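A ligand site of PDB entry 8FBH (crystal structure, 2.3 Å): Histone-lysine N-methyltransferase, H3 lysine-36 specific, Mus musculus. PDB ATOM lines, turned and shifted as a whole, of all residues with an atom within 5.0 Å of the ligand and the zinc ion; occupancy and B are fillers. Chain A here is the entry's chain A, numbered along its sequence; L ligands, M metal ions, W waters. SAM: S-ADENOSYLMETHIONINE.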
ATOM      1  N   GLN A 101     -32.511 -33.984 -24.366  1.00  0.00           N
ATOM      2  CA  GLN A 101     -32.941 -34.293 -22.986  1.00  0.00           C
ATOM      3  C   GLN A 101     -32.732 -33.098 -22.029  1.00  0.00           C
ATOM      4  O   GLN A 101     -33.129 -33.226 -20.863  1.00  0.00           O
ATOM      5  CB  GLN A 101     -32.117 -35.488 -22.503  1.00  0.00           C
ATOM      6  CG  GLN A 101     -32.597 -36.832 -23.052  1.00  0.00           C
ATOM      7  CD  GLN A 101     -32.131 -37.980 -22.181  1.00  0.00           C
ATOM      8  OE1 GLN A 101     -30.964 -38.349 -22.196  1.00  0.00           O
ATOM      9  NE2 GLN A 101     -33.050 -38.519 -21.373  1.00  0.00           N
ATOM     10  N   ARG A 102     -32.086 -32.012 -22.463  1.00  0.00           N
ATOM     11  CA  ARG A 102     -31.612 -30.918 -21.579  1.00  0.00           C
ATOM     12  C   ARG A 102     -32.031 -29.580 -22.173  1.00  0.00           C
ATOM     13  O   ARG A 102     -31.297 -28.579 -21.993  1.00  0.00           O
ATOM     14  CB  ARG A 102     -30.085 -30.998 -21.375  1.00  0.00           C
ATOM     15  CG  ARG A 102     -29.626 -32.188 -20.560  1.00  0.00           C
ATOM     16  CD  ARG A 102     -28.132 -32.485 -20.641  1.00  0.00           C
ATOM     17  NE  ARG A 102     -27.739 -32.694 -22.034  1.00  0.00           N
ATOM     18  CZ  ARG A 102     -26.947 -31.906 -22.736  1.00  0.00           C
ATOM     19  NH1 ARG A 102     -26.359 -30.858 -22.167  1.00  0.00           N
ATOM     20  NH2 ARG A 102     -26.729 -32.176 -24.001  1.00  0.00           N
ATOM     21  N   GLY A 103     -33.150 -29.555 -22.899  1.00  0.00           N
ATOM     22  CA  GLY A 103     -33.705 -28.320 -23.488  1.00  0.00           C
ATOM     23  C   GLY A 103     -32.738 -27.670 -24.463  1.00  0.00           C
ATOM     24  O   GLY A 103     -32.167 -28.416 -25.282  1.00  0.00           O
ATOM     25  N   TRP A 104     -32.653 -26.343 -24.451  1.00  0.00           N
ATOM     26  CA  TRP A 104     -31.705 -25.550 -25.272  1.00  0.00           C
ATOM     27  C   TRP A 104     -30.336 -25.524 -24.562  1.00  0.00           C
ATOM     28  O   TRP A 104     -30.319 -25.461 -23.324  1.00  0.00           O
ATOM     29  CB  TRP A 104     -32.236 -24.137 -25.485  1.00  0.00           C
ATOM     30  CG  TRP A 104     -33.502 -24.110 -26.282  1.00  0.00           C
ATOM     31  CD1 TRP A 104     -34.776 -24.174 -25.813  1.00  0.00           C
ATOM     32  CD2 TRP A 104     -33.614 -24.067 -27.718  1.00  0.00           C
ATOM     33  NE1 TRP A 104     -35.677 -24.172 -26.840  1.00  0.00           N
ATOM     34  CE2 TRP A 104     -34.986 -24.100 -28.017  1.00  0.00           C
ATOM     35  CE3 TRP A 104     -32.682 -24.017 -28.760  1.00  0.00           C
ATOM     36  CZ2 TRP A 104     -35.452 -24.072 -29.328  1.00  0.00           C
ATOM     37  CZ3 TRP A 104     -33.144 -23.981 -30.050  1.00  0.00           C
ATOM     38  CH2 TRP A 104     -34.511 -24.017 -30.330  1.00  0.00           C
ATOM     39  N   TYR A 121     -22.293 -14.704 -15.637  1.00  0.00           N
ATOM     40  CA  TYR A 121     -23.673 -15.127 -15.359  1.00  0.00           C
ATOM     41  C   TYR A 121     -24.450 -13.898 -14.860  1.00  0.00           C
ATOM     42  O   TYR A 121     -24.332 -13.521 -13.679  1.00  0.00           O
ATOM     43  CB  TYR A 121     -23.734 -16.301 -14.386  1.00  0.00           C
ATOM     44  CG  TYR A 121     -25.052 -17.027 -14.413  1.00  0.00           C
ATOM     45  CD1 TYR A 121     -25.253 -18.084 -15.278  1.00  0.00           C
ATOM     46  CD2 TYR A 121     -26.111 -16.625 -13.625  1.00  0.00           C
ATOM     47  CE1 TYR A 121     -26.480 -18.722 -15.373  1.00  0.00           C
ATOM     48  CE2 TYR A 121     -27.335 -17.280 -13.681  1.00  0.00           C
ATOM     49  CZ  TYR A 121     -27.529 -18.310 -14.576  1.00  0.00           C
ATOM     50  OH  TYR A 121     -28.716 -18.966 -14.653  1.00  0.00           O
ATOM     51  N   THR A 144     -39.811 -26.633 -15.089  1.00  0.00           N
ATOM     52  CA  THR A 144     -38.621 -27.318 -14.514  1.00  0.00           C
ATOM     53  C   THR A 144     -37.315 -26.620 -14.941  1.00  0.00           C
ATOM     54  O   THR A 144     -36.247 -27.064 -14.483  1.00  0.00           O
ATOM     55  CB  THR A 144     -38.580 -28.815 -14.885  1.00  0.00           C
ATOM     56  OG1 THR A 144     -38.839 -28.977 -16.276  1.00  0.00           O
ATOM     57  CG2 THR A 144     -39.570 -29.640 -14.087  1.00  0.00           C
ATOM     58  N   ASN A 145     -37.407 -25.554 -15.737  1.00  0.00           N
ATOM     59  CA  ASN A 145     -36.243 -24.703 -16.108  1.00  0.00           C
ATOM     60  C   ASN A 145     -36.074 -23.603 -15.058  1.00  0.00           C
ATOM     61  O   ASN A 145     -36.917 -22.699 -15.009  1.00  0.00           O
ATOM     62  CB  ASN A 145     -36.393 -24.133 -17.529  1.00  0.00           C
ATOM     63  CG  ASN A 145     -36.037 -25.157 -18.567  1.00  0.00           C
ATOM     64  OD1 ASN A 145     -35.026 -25.847 -18.425  1.00  0.00           O
ATOM     65  ND2 ASN A 145     -36.864 -25.300 -19.585  1.00  0.00           N
ATOM     66  N   PHE A 146     -34.960 -23.641 -14.323  1.00  0.00           N
ATOM     67  CA  PHE A 146     -34.556 -22.621 -13.323  1.00  0.00           C
ATOM     68  C   PHE A 146     -33.230 -21.986 -13.723  1.00  0.00           C
ATOM     69  O   PHE A 146     -32.365 -22.662 -14.304  1.00  0.00           O
ATOM     70  CB  PHE A 146     -34.446 -23.251 -11.941  1.00  0.00           C
ATOM     71  CG  PHE A 146     -35.714 -23.885 -11.443  1.00  0.00           C
ATOM     72  CD1 PHE A 146     -36.722 -23.112 -10.889  1.00  0.00           C
ATOM     73  CD2 PHE A 146     -35.940 -25.245 -11.608  1.00  0.00           C
ATOM     74  CE1 PHE A 146     -37.889 -23.690 -10.445  1.00  0.00           C
ATOM     75  CE2 PHE A 146     -37.131 -25.824 -11.177  1.00  0.00           C
ATOM     76  CZ  PHE A 146     -38.099 -25.051 -10.593  1.00  0.00           C
ATOM     77  N   TYR A 147     -33.039 -20.729 -13.373  1.00  0.00           N
ATOM     78  CA  TYR A 147     -31.883 -19.903 -13.830  1.00  0.00           C
ATOM     79  C   TYR A 147     -31.274 -19.177 -12.641  1.00  0.00           C
ATOM     80  O   TYR A 147     -30.523 -18.184 -12.836  1.00  0.00           O
ATOM     81  CB  TYR A 147     -32.340 -18.938 -14.921  1.00  0.00           C
ATOM     82  CG  TYR A 147     -32.962 -19.613 -16.121  1.00  0.00           C
ATOM     83  CD1 TYR A 147     -34.332 -19.857 -16.178  1.00  0.00           C
ATOM     84  CD2 TYR A 147     -32.181 -19.977 -17.210  1.00  0.00           C
ATOM     85  CE1 TYR A 147     -34.913 -20.417 -17.299  1.00  0.00           C
ATOM     86  CE2 TYR A 147     -32.743 -20.568 -18.320  1.00  0.00           C
ATOM     87  CZ  TYR A 147     -34.108 -20.781 -18.374  1.00  0.00           C
ATOM     88  OH  TYR A 147     -34.648 -21.403 -19.464  1.00  0.00           O
ATOM     89  N   ARG A 167     -27.069 -18.080 -19.646  1.00  0.00           N
ATOM     90  CA  ARG A 167     -28.289 -18.718 -19.090  1.00  0.00           C
ATOM     91  C   ARG A 167     -28.601 -20.020 -19.842  1.00  0.00           C
ATOM     92  O   ARG A 167     -29.489 -20.722 -19.394  1.00  0.00           O
ATOM     93  CB  ARG A 167     -29.506 -17.780 -19.187  1.00  0.00           C
ATOM     94  CG  ARG A 167     -30.043 -17.658 -20.611  1.00  0.00           C
ATOM     95  CD  ARG A 167     -30.918 -16.446 -20.844  1.00  0.00           C
ATOM     96  NE  ARG A 167     -32.236 -16.568 -20.266  1.00  0.00           N
ATOM     97  CZ  ARG A 167     -33.204 -17.330 -20.741  1.00  0.00           C
ATOM     98  NH1 ARG A 167     -34.380 -17.358 -20.118  1.00  0.00           N
ATOM     99  NH2 ARG A 167     -32.993 -18.091 -21.813  1.00  0.00           N
ATOM    100  N   PHE A 168     -27.976 -20.271 -20.995  1.00  0.00           N
ATOM    101  CA  PHE A 168     -28.281 -21.438 -21.855  1.00  0.00           C
ATOM    102  C   PHE A 168     -27.267 -22.571 -21.600  1.00  0.00           C
ATOM    103  O   PHE A 168     -27.358 -23.608 -22.274  1.00  0.00           O
ATOM    104  CB  PHE A 168     -28.309 -21.034 -23.337  1.00  0.00           C
ATOM    105  CG  PHE A 168     -29.556 -20.302 -23.773  1.00  0.00           C
ATOM    106  CD1 PHE A 168     -30.741 -20.977 -24.012  1.00  0.00           C
ATOM    107  CD2 PHE A 168     -29.542 -18.927 -23.953  1.00  0.00           C
ATOM    108  CE1 PHE A 168     -31.892 -20.300 -24.410  1.00  0.00           C
ATOM    109  CE2 PHE A 168     -30.697 -18.236 -24.317  1.00  0.00           C
ATOM    110  CZ  PHE A 168     -31.866 -18.923 -24.541  1.00  0.00           C
ATOM    111  N   MET A 169     -26.339 -22.389 -20.649  1.00  0.00           N
ATOM    112  CA  MET A 169     -25.240 -23.358 -20.384  1.00  0.00           C
ATOM    113  C   MET A 169     -25.728 -24.441 -19.406  1.00  0.00           C
ATOM    114  O   MET A 169     -26.126 -24.126 -18.302  1.00  0.00           O
ATOM    115  CB  MET A 169     -23.992 -22.638 -19.841  1.00  0.00           C
ATOM    116  CG  MET A 169     -23.333 -21.765 -20.932  1.00  0.00           C
ATOM    117  SD  MET A 169     -21.790 -20.979 -20.457  1.00  0.00           S
ATOM    118  CE  MET A 169     -20.912 -22.388 -19.779  1.00  0.00           C
ATOM    119  N   ASN A 170     -25.761 -25.686 -19.865  1.00  0.00           N
ATOM    120  CA  ASN A 170     -26.326 -26.824 -19.093  1.00  0.00           C
ATOM    121  C   ASN A 170     -25.310 -27.326 -18.049  1.00  0.00           C
ATOM    122  O   ASN A 170     -24.088 -27.032 -18.151  1.00  0.00           O
ATOM    123  CB  ASN A 170     -26.807 -27.925 -20.050  1.00  0.00           C
ATOM    124  CG  ASN A 170     -28.081 -27.562 -20.784  1.00  0.00           C
ATOM    125  OD1 ASN A 170     -28.994 -27.008 -20.196  1.00  0.00           O
ATOM    126  ND2 ASN A 170     -28.167 -27.873 -22.070  1.00  0.00           N
ATOM    127  N   HIS A 171     -25.793 -28.042 -17.050  1.00  0.00           N
ATOM    128  CA  HIS A 171     -24.934 -28.705 -16.045  1.00  0.00           C
ATOM    129  C   HIS A 171     -24.298 -29.933 -16.713  1.00  0.00           C
ATOM    130  O   HIS A 171     -24.967 -30.658 -17.420  1.00  0.00           O
ATOM    131  CB  HIS A 171     -25.726 -29.151 -14.819  1.00  0.00           C
ATOM    132  CG  HIS A 171     -24.986 -30.174 -14.011  1.00  0.00           C
ATOM    133  ND1 HIS A 171     -24.002 -29.819 -13.115  1.00  0.00           N
ATOM    134  CD2 HIS A 171     -25.016 -31.522 -14.032  1.00  0.00           C
ATOM    135  CE1 HIS A 171     -23.448 -30.912 -12.620  1.00  0.00           C
ATOM    136  NE2 HIS A 171     -24.049 -31.967 -13.165  1.00  0.00           N
ATOM    137  N   CYS A 172     -23.057 -30.212 -16.388  1.00  0.00           N
ATOM    138  CA  CYS A 172     -22.439 -31.493 -16.689  1.00  0.00           C
ATOM    139  C   CYS A 172     -21.594 -31.894 -15.505  1.00  0.00           C
ATOM    140  O   CYS A 172     -21.087 -30.981 -14.826  1.00  0.00           O
ATOM    141  CB  CYS A 172     -21.604 -31.397 -17.938  1.00  0.00           C
ATOM    142  SG  CYS A 172     -20.710 -32.918 -18.220  1.00  0.00           S
ATOM    143  N   CYS A 173     -21.494 -33.213 -15.255  1.00  0.00           N
ATOM    144  CA  CYS A 173     -20.620 -33.798 -14.212  1.00  0.00           C
ATOM    145  C   CYS A 173     -19.197 -33.963 -14.769  1.00  0.00           C
ATOM    146  O   CYS A 173     -18.274 -34.105 -13.960  1.00  0.00           O
ATOM    147  CB  CYS A 173     -21.158 -35.135 -13.720  1.00  0.00           C
ATOM    148  SG  CYS A 173     -22.872 -35.051 -13.130  1.00  0.00           S
ATOM    149  N   TYR A 208     -22.947 -27.172 -11.934  1.00  0.00           N
ATOM    150  CA  TYR A 208     -23.860 -26.272 -11.169  1.00  0.00           C
ATOM    151  C   TYR A 208     -23.481 -26.315  -9.686  1.00  0.00           C
ATOM    152  O   TYR A 208     -23.718 -25.340  -8.944  1.00  0.00           O
ATOM    153  CB  TYR A 208     -25.325 -26.650 -11.406  1.00  0.00           C
ATOM    154  CG  TYR A 208     -25.913 -26.246 -12.731  1.00  0.00           C
ATOM    155  CD1 TYR A 208     -25.127 -25.784 -13.774  1.00  0.00           C
ATOM    156  CD2 TYR A 208     -27.257 -26.407 -12.984  1.00  0.00           C
ATOM    157  CE1 TYR A 208     -25.662 -25.471 -15.012  1.00  0.00           C
ATOM    158  CE2 TYR A 208     -27.816 -26.129 -14.220  1.00  0.00           C
ATOM    159  CZ  TYR A 208     -27.018 -25.649 -15.243  1.00  0.00           C
ATOM    160  OH  TYR A 208     -27.584 -25.339 -16.440  1.00  0.00           O
ATOM    161  N   CYS A 212     -27.976 -24.312  -8.589  1.00  0.00           N
ATOM    162  CA  CYS A 212     -29.168 -23.933  -9.398  1.00  0.00           C
ATOM    163  C   CYS A 212     -30.424 -24.149  -8.547  1.00  0.00           C
ATOM    164  O   CYS A 212     -30.871 -25.303  -8.404  1.00  0.00           O
ATOM    165  CB  CYS A 212     -29.244 -24.690 -10.710  1.00  0.00           C
ATOM    166  SG  CYS A 212     -30.205 -23.791 -11.955  1.00  0.00           S
ATOM    167  N   ASN A 215     -33.512 -26.928  -8.525  1.00  0.00           N
ATOM    168  CA  ASN A 215     -33.149 -28.177  -9.240  1.00  0.00           C
ATOM    169  C   ASN A 215     -32.702 -29.260  -8.237  1.00  0.00           C
ATOM    170  O   ASN A 215     -32.131 -30.233  -8.679  1.00  0.00           O
ATOM    171  CB  ASN A 215     -32.101 -27.907 -10.317  1.00  0.00           C
ATOM    172  CG  ASN A 215     -32.737 -27.443 -11.618  1.00  0.00           C
ATOM    173  OD1 ASN A 215     -32.389 -26.370 -12.112  1.00  0.00           O
ATOM    174  ND2 ASN A 215     -33.664 -28.219 -12.150  1.00  0.00           N
ATOM    175  N   THR A 218     -33.473 -32.869  -9.119  1.00  0.00           N
ATOM    176  CA  THR A 218     -33.487 -33.102 -10.593  1.00  0.00           C
ATOM    177  C   THR A 218     -32.497 -34.222 -10.961  1.00  0.00           C
ATOM    178  O   THR A 218     -31.354 -34.249 -10.422  1.00  0.00           O
ATOM    179  CB  THR A 218     -33.219 -31.820 -11.381  1.00  0.00           C
ATOM    180  OG1 THR A 218     -34.092 -30.806 -10.853  1.00  0.00           O
ATOM    181  CG2 THR A 218     -33.432 -31.977 -12.869  1.00  0.00           C
ATOM    182  N   VAL A 219     -32.914 -35.123 -11.844  1.00  0.00           N
ATOM    183  CA  VAL A 219     -32.035 -36.232 -12.303  1.00  0.00           C
ATOM    184  C   VAL A 219     -31.147 -35.672 -13.404  1.00  0.00           C
ATOM    185  O   VAL A 219     -31.668 -35.057 -14.328  1.00  0.00           O
ATOM    186  CB  VAL A 219     -32.829 -37.459 -12.794  1.00  0.00           C
ATOM    187  CG1 VAL A 219     -31.914 -38.477 -13.483  1.00  0.00           C
ATOM    188  CG2 VAL A 219     -33.635 -38.116 -11.658  1.00  0.00           C
ATOM    189  N   CYS A 220     -29.849 -35.900 -13.301  1.00  0.00           N
ATOM    190  CA  CYS A 220     -28.886 -35.403 -14.286  1.00  0.00           C
ATOM    191  C   CYS A 220     -28.974 -36.287 -15.540  1.00  0.00           C
ATOM    192  O   CYS A 220     -29.040 -37.498 -15.393  1.00  0.00           O
ATOM    193  CB  CYS A 220     -27.468 -35.394 -13.719  1.00  0.00           C
ATOM    194  SG  CYS A 220     -26.312 -34.646 -14.895  1.00  0.00           S
ATOM    195  N   LYS A 221     -28.976 -35.668 -16.724  1.00  0.00           N
ATOM    196  CA  LYS A 221     -28.945 -36.370 -18.028  1.00  0.00           C
ATOM    197  C   LYS A 221     -27.645 -36.057 -18.762  1.00  0.00           C
ATOM    198  O   LYS A 221     -27.682 -36.129 -19.964  1.00  0.00           O
ATOM    199  CB  LYS A 221     -30.114 -35.942 -18.911  1.00  0.00           C
ATOM    200  CG  LYS A 221     -31.492 -36.132 -18.293  1.00  0.00           C
ATOM    201  CD  LYS A 221     -31.858 -37.587 -18.071  1.00  0.00           C
ATOM    202  CE  LYS A 221     -33.224 -37.785 -17.458  1.00  0.00           C
ATOM    203  NZ  LYS A 221     -33.512 -39.214 -17.203  1.00  0.00           N
ATOM    204  N   CYS A 222     -26.563 -35.679 -18.072  1.00  0.00           N
ATOM    205  CA  CYS A 222     -25.319 -35.220 -18.747  1.00  0.00           C
ATOM    206  C   CYS A 222     -24.704 -36.389 -19.526  1.00  0.00           C
ATOM    207  O   CYS A 222     -24.040 -36.108 -20.528  1.00  0.00           O
ATOM    208  CB  CYS A 222     -24.303 -34.583 -17.798  1.00  0.00           C
ATOM    209  SG  CYS A 222     -23.410 -35.720 -16.705  1.00  0.00           S
ATOM    210  N   GLY A 223     -24.943 -37.636 -19.111  1.00  0.00           N
ATOM    211  CA  GLY A 223     -24.506 -38.867 -19.814  1.00  0.00           C
ATOM    212  C   GLY A 223     -23.006 -39.146 -19.662  1.00  0.00           C
ATOM    213  O   GLY A 223     -22.471 -39.909 -20.473  1.00  0.00           O
ATOM    214  N   CYS A 227     -21.177 -39.557 -13.755  1.00  0.00           N
ATOM    215  CA  CYS A 227     -22.377 -38.725 -13.441  1.00  0.00           C
ATOM    216  C   CYS A 227     -22.827 -39.026 -12.011  1.00  0.00           C
ATOM    217  O   CYS A 227     -22.997 -40.205 -11.681  1.00  0.00           O
ATOM    218  CB  CYS A 227     -23.501 -38.998 -14.441  1.00  0.00           C
ATOM    219  SG  CYS A 227     -25.039 -38.105 -14.121  1.00  0.00           S
ATOM    220  N   SER A 228     -23.016 -37.985 -11.200  1.00  0.00           N
ATOM    221  CA  SER A 228     -23.490 -38.080  -9.785  1.00  0.00           C
ATOM    222  C   SER A 228     -24.970 -38.508  -9.720  1.00  0.00           C
ATOM    223  O   SER A 228     -25.427 -38.849  -8.621  1.00  0.00           O
ATOM    224  CB  SER A 228     -23.295 -36.763  -9.101  1.00  0.00           C
ATOM    225  OG  SER A 228     -24.159 -35.788  -9.699  1.00  0.00           O
ATOM    226  N   GLY A 229     -25.708 -38.374 -10.828  1.00  0.00           N
ATOM    227  CA  GLY A 229     -27.186 -38.498 -10.846  1.00  0.00           C
ATOM    228  C   GLY A 229     -27.939 -37.178 -10.583  1.00  0.00           C
ATOM    229  O   GLY A 229     -29.163 -37.163 -10.804  1.00  0.00           O
ATOM    230  N   PHE A 230     -27.257 -36.109 -10.156  1.00  0.00           N
ATOM    231  CA  PHE A 230     -27.876 -34.830  -9.739  1.00  0.00           C
ATOM    232  C   PHE A 230     -27.104 -33.626 -10.320  1.00  0.00           C
ATOM    233  O   PHE A 230     -25.977 -33.793 -10.884  1.00  0.00           O
ATOM    234  CB  PHE A 230     -28.002 -34.781  -8.218  1.00  0.00           C
ATOM    235  CG  PHE A 230     -26.763 -35.064  -7.398  1.00  0.00           C
ATOM    236  CD1 PHE A 230     -25.818 -34.066  -7.144  1.00  0.00           C
ATOM    237  CD2 PHE A 230     -26.590 -36.299  -6.778  1.00  0.00           C
ATOM    238  CE1 PHE A 230     -24.729 -34.313  -6.305  1.00  0.00           C
ATOM    239  CE2 PHE A 230     -25.501 -36.546  -5.939  1.00  0.00           C
ATOM    240  CZ  PHE A 230     -24.562 -35.546  -5.704  1.00  0.00           C
ATOM    241  N   LEU A 231     -27.691 -32.432 -10.242  1.00  0.00           N
ATOM    242  CA  LEU A 231     -27.079 -31.214 -10.858  1.00  0.00           C
ATOM    243  C   LEU A 231     -25.987 -30.689  -9.906  1.00  0.00           C
ATOM    244  O   LEU A 231     -26.041 -29.491  -9.491  1.00  0.00           O
ATOM    245  CB  LEU A 231     -28.173 -30.193 -11.180  1.00  0.00           C
ATOM    246  CG  LEU A 231     -29.249 -30.645 -12.178  1.00  0.00           C
ATOM    247  CD1 LEU A 231     -29.873 -29.456 -12.901  1.00  0.00           C
ATOM    248  CD2 LEU A 231     -28.705 -31.624 -13.193  1.00  0.00           C
HETATM  249  N   SAM L   1     -31.497 -26.073 -20.836  1.00  0.00           N
HETATM  250  CA  SAM L   1     -31.904 -24.738 -20.337  1.00  0.00           C
HETATM  251  C   SAM L   1     -32.952 -24.113 -21.291  1.00  0.00           C
HETATM  252  O   SAM L   1     -33.534 -24.887 -22.105  1.00  0.00           O
HETATM  253  OXT SAM L   1     -33.168 -22.890 -21.182  1.00  0.00           O
HETATM  254  CB  SAM L   1     -30.664 -23.857 -20.210  1.00  0.00           C
HETATM  255  CG  SAM L   1     -29.915 -24.063 -18.884  1.00  0.00           C
HETATM  256  SD  SAM L   1     -30.909 -23.405 -17.508  1.00  0.00           S
HETATM  257  CE  SAM L   1     -29.729 -22.322 -16.711  1.00  0.00           C
HETATM  258  C5' SAM L   1     -30.919 -24.792 -16.349  1.00  0.00           C
HETATM  259  C4' SAM L   1     -32.020 -25.808 -16.569  1.00  0.00           C
HETATM  260  O4' SAM L   1     -31.650 -26.697 -17.655  1.00  0.00           O
HETATM  261  C3' SAM L   1     -32.286 -26.715 -15.379  1.00  0.00           C
HETATM  262  O3' SAM L   1     -33.202 -26.096 -14.485  1.00  0.00           O
HETATM  263  C2' SAM L   1     -32.818 -27.980 -16.059  1.00  0.00           C
HETATM  264  O2' SAM L   1     -34.186 -27.896 -16.374  1.00  0.00           O
HETATM  265  C1' SAM L   1     -31.982 -28.041 -17.343  1.00  0.00           C
HETATM  266  N9  SAM L   1     -30.735 -28.802 -17.239  1.00  0.00           N
HETATM  267  C8  SAM L   1     -29.471 -28.288 -17.332  1.00  0.00           C
HETATM  268  N7  SAM L   1     -28.526 -29.194 -17.243  1.00  0.00           N
HETATM  269  C5  SAM L   1     -29.211 -30.397 -17.078  1.00  0.00           C
HETATM  270  C6  SAM L   1     -28.768 -31.728 -16.933  1.00  0.00           C
HETATM  271  N6  SAM L   1     -27.492 -32.093 -16.937  1.00  0.00           N
HETATM  272  N1  SAM L   1     -29.704 -32.680 -16.771  1.00  0.00           N
HETATM  273  C2  SAM L   1     -30.994 -32.314 -16.783  1.00  0.00           C
HETATM  274  N3  SAM L   1     -31.526 -31.113 -16.962  1.00  0.00           N
HETATM  275  C4  SAM L   1     -30.568 -30.175 -17.091  1.00  0.00           C
HETATM  276 ZN    ZN M   1     -24.427 -35.805 -14.640  1.00  0.00          ZN
HETATM  277  O   HOH W   1     -34.033 -27.434 -20.106  1.00  0.00           O
HETATM  278  O   HOH W   2     -36.174 -25.839 -22.191  1.00  0.00           O
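Water W2 bridges the side-chain amide nitrogen of Asn 145 (2.7 Å) and an oxygen (O) of the ligand (2.8 Å). Water W1 lies within hydrogen-bond range of OD1 of Asn 145 and N of the ligand.
The side-chain sulfur (SG) of Cys 173 sits close to a ring nitrogen (NE2) of His 171 (3.3 Å). OD1 of Asn 215 sits at hydrogen-bond distance from SG of Cys 212 (3.4 Å). ND2 of Asn 215 sits at hydrogen-bond distance from OG1 of Thr 218 (2.9 Å). The side-chain amide nitrogen (ND2) of Asn 170 sits at hydrogen-bond distance from the backbone carbonyl oxygen (O) of Arg 102, at 3.2 Å. The backbone carbonyl oxygen (O) of Phe 146 sits at hydrogen-bond distance from the side-chain sulfur (SG) of Cys 212. The backbone carbonyl oxygen (O) of Trp 104 sits at hydrogen-bond distance from the side-chain amide nitrogen (ND2) of Asn 170 (3.5 Å). SG of Cys 227 lies close to N of Gly 229, at 3.4 Å. The backbone NH of Cys 220 sits at hydrogen-bond distance from the backbone carbonyl oxygen of Gly 229.
The backbone carbonyl oxygen (O) of Arg 102 is in hydrogen-bond range of a nitrogen (N) of the ligand. The side-chain amide oxygen of Asn 145 lies within hydrogen-bond range of an oxygen (O2') of the ligand. The side-chain sulfur (SG) of Cys 220 lies close to a nitrogen (N6) of the ligand (3.5 Å). The backbone NH of Lys 221 sits at hydrogen-bond distance from a nitrogen (N1) of the ligand, 3.1 Å away. The side-chain hydroxyl (OH) of Tyr 147 lies within hydrogen-bond range of an oxygen (OXT) of the ligand (2.7 Å). The backbone NH of Phe 146 lies within hydrogen-bond range of an oxygen (O3') of the ligand (3.0 Å). OD1 of Asn 215 lies within hydrogen-bond range of O3' of the ligand. The backbone carbonyl oxygen of Thr 144 sits at hydrogen-bond distance from an oxygen (O2') of the ligand (2.9 Å). The backbone NH (N) of Trp 104 lies within hydrogen-bond range of an oxygen (O) of the ligand (2.9 Å). A nitrogen (N6) of the ligand is in hydrogen-bond range of the backbone carbonyl oxygen (O) of His 171 (2.9 Å). A nitrogen (N7) of the ligand lies within hydrogen-bond range of the backbone NH of His 171, 3.0 Å away. O of Trp 104 is in hydrogen-bond range of N of the ligand, at 2.8 Å. A nitrogen (N) of the ligand sits at hydrogen-bond distance from the side-chain amide oxygen (OD1) of Asn 170, at 2.7 Å.
The zinc ion is bound by SG of Cys 220 (2.2 Å), SG of Cys 173 (2.3 Å), SG of Cys 222 (2.3 Å) and SG of Cys 227 (2.4 Å).
Of the 30 residues printed, 4 come within 4 Å of the zinc ion.
A sulfur (SD) of the ligand lies close to the backbone carbonyl oxygen (O) of Arg 167. Gly 103 touches the ligand. Phe 168 touches the ligand (CA to CB, 3.8 Å). Met 169 touches the ligand. OH of Tyr 208 touches C5' of the ligand (3.4 Å). Val 219 touches the ligand. Leu 231 touches the ligand (CD2 to C6, 3.7 Å). Hydrophobic or aromatic side chains that line the ligand: Trp 104, Tyr 147, His 171, Tyr 208 and Leu 231. Of the 30 residues printed, 19 come within 4 Å of the ligand. The nearest printed residue that does not touch the ligand is Tyr 121 (4.1 Å).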
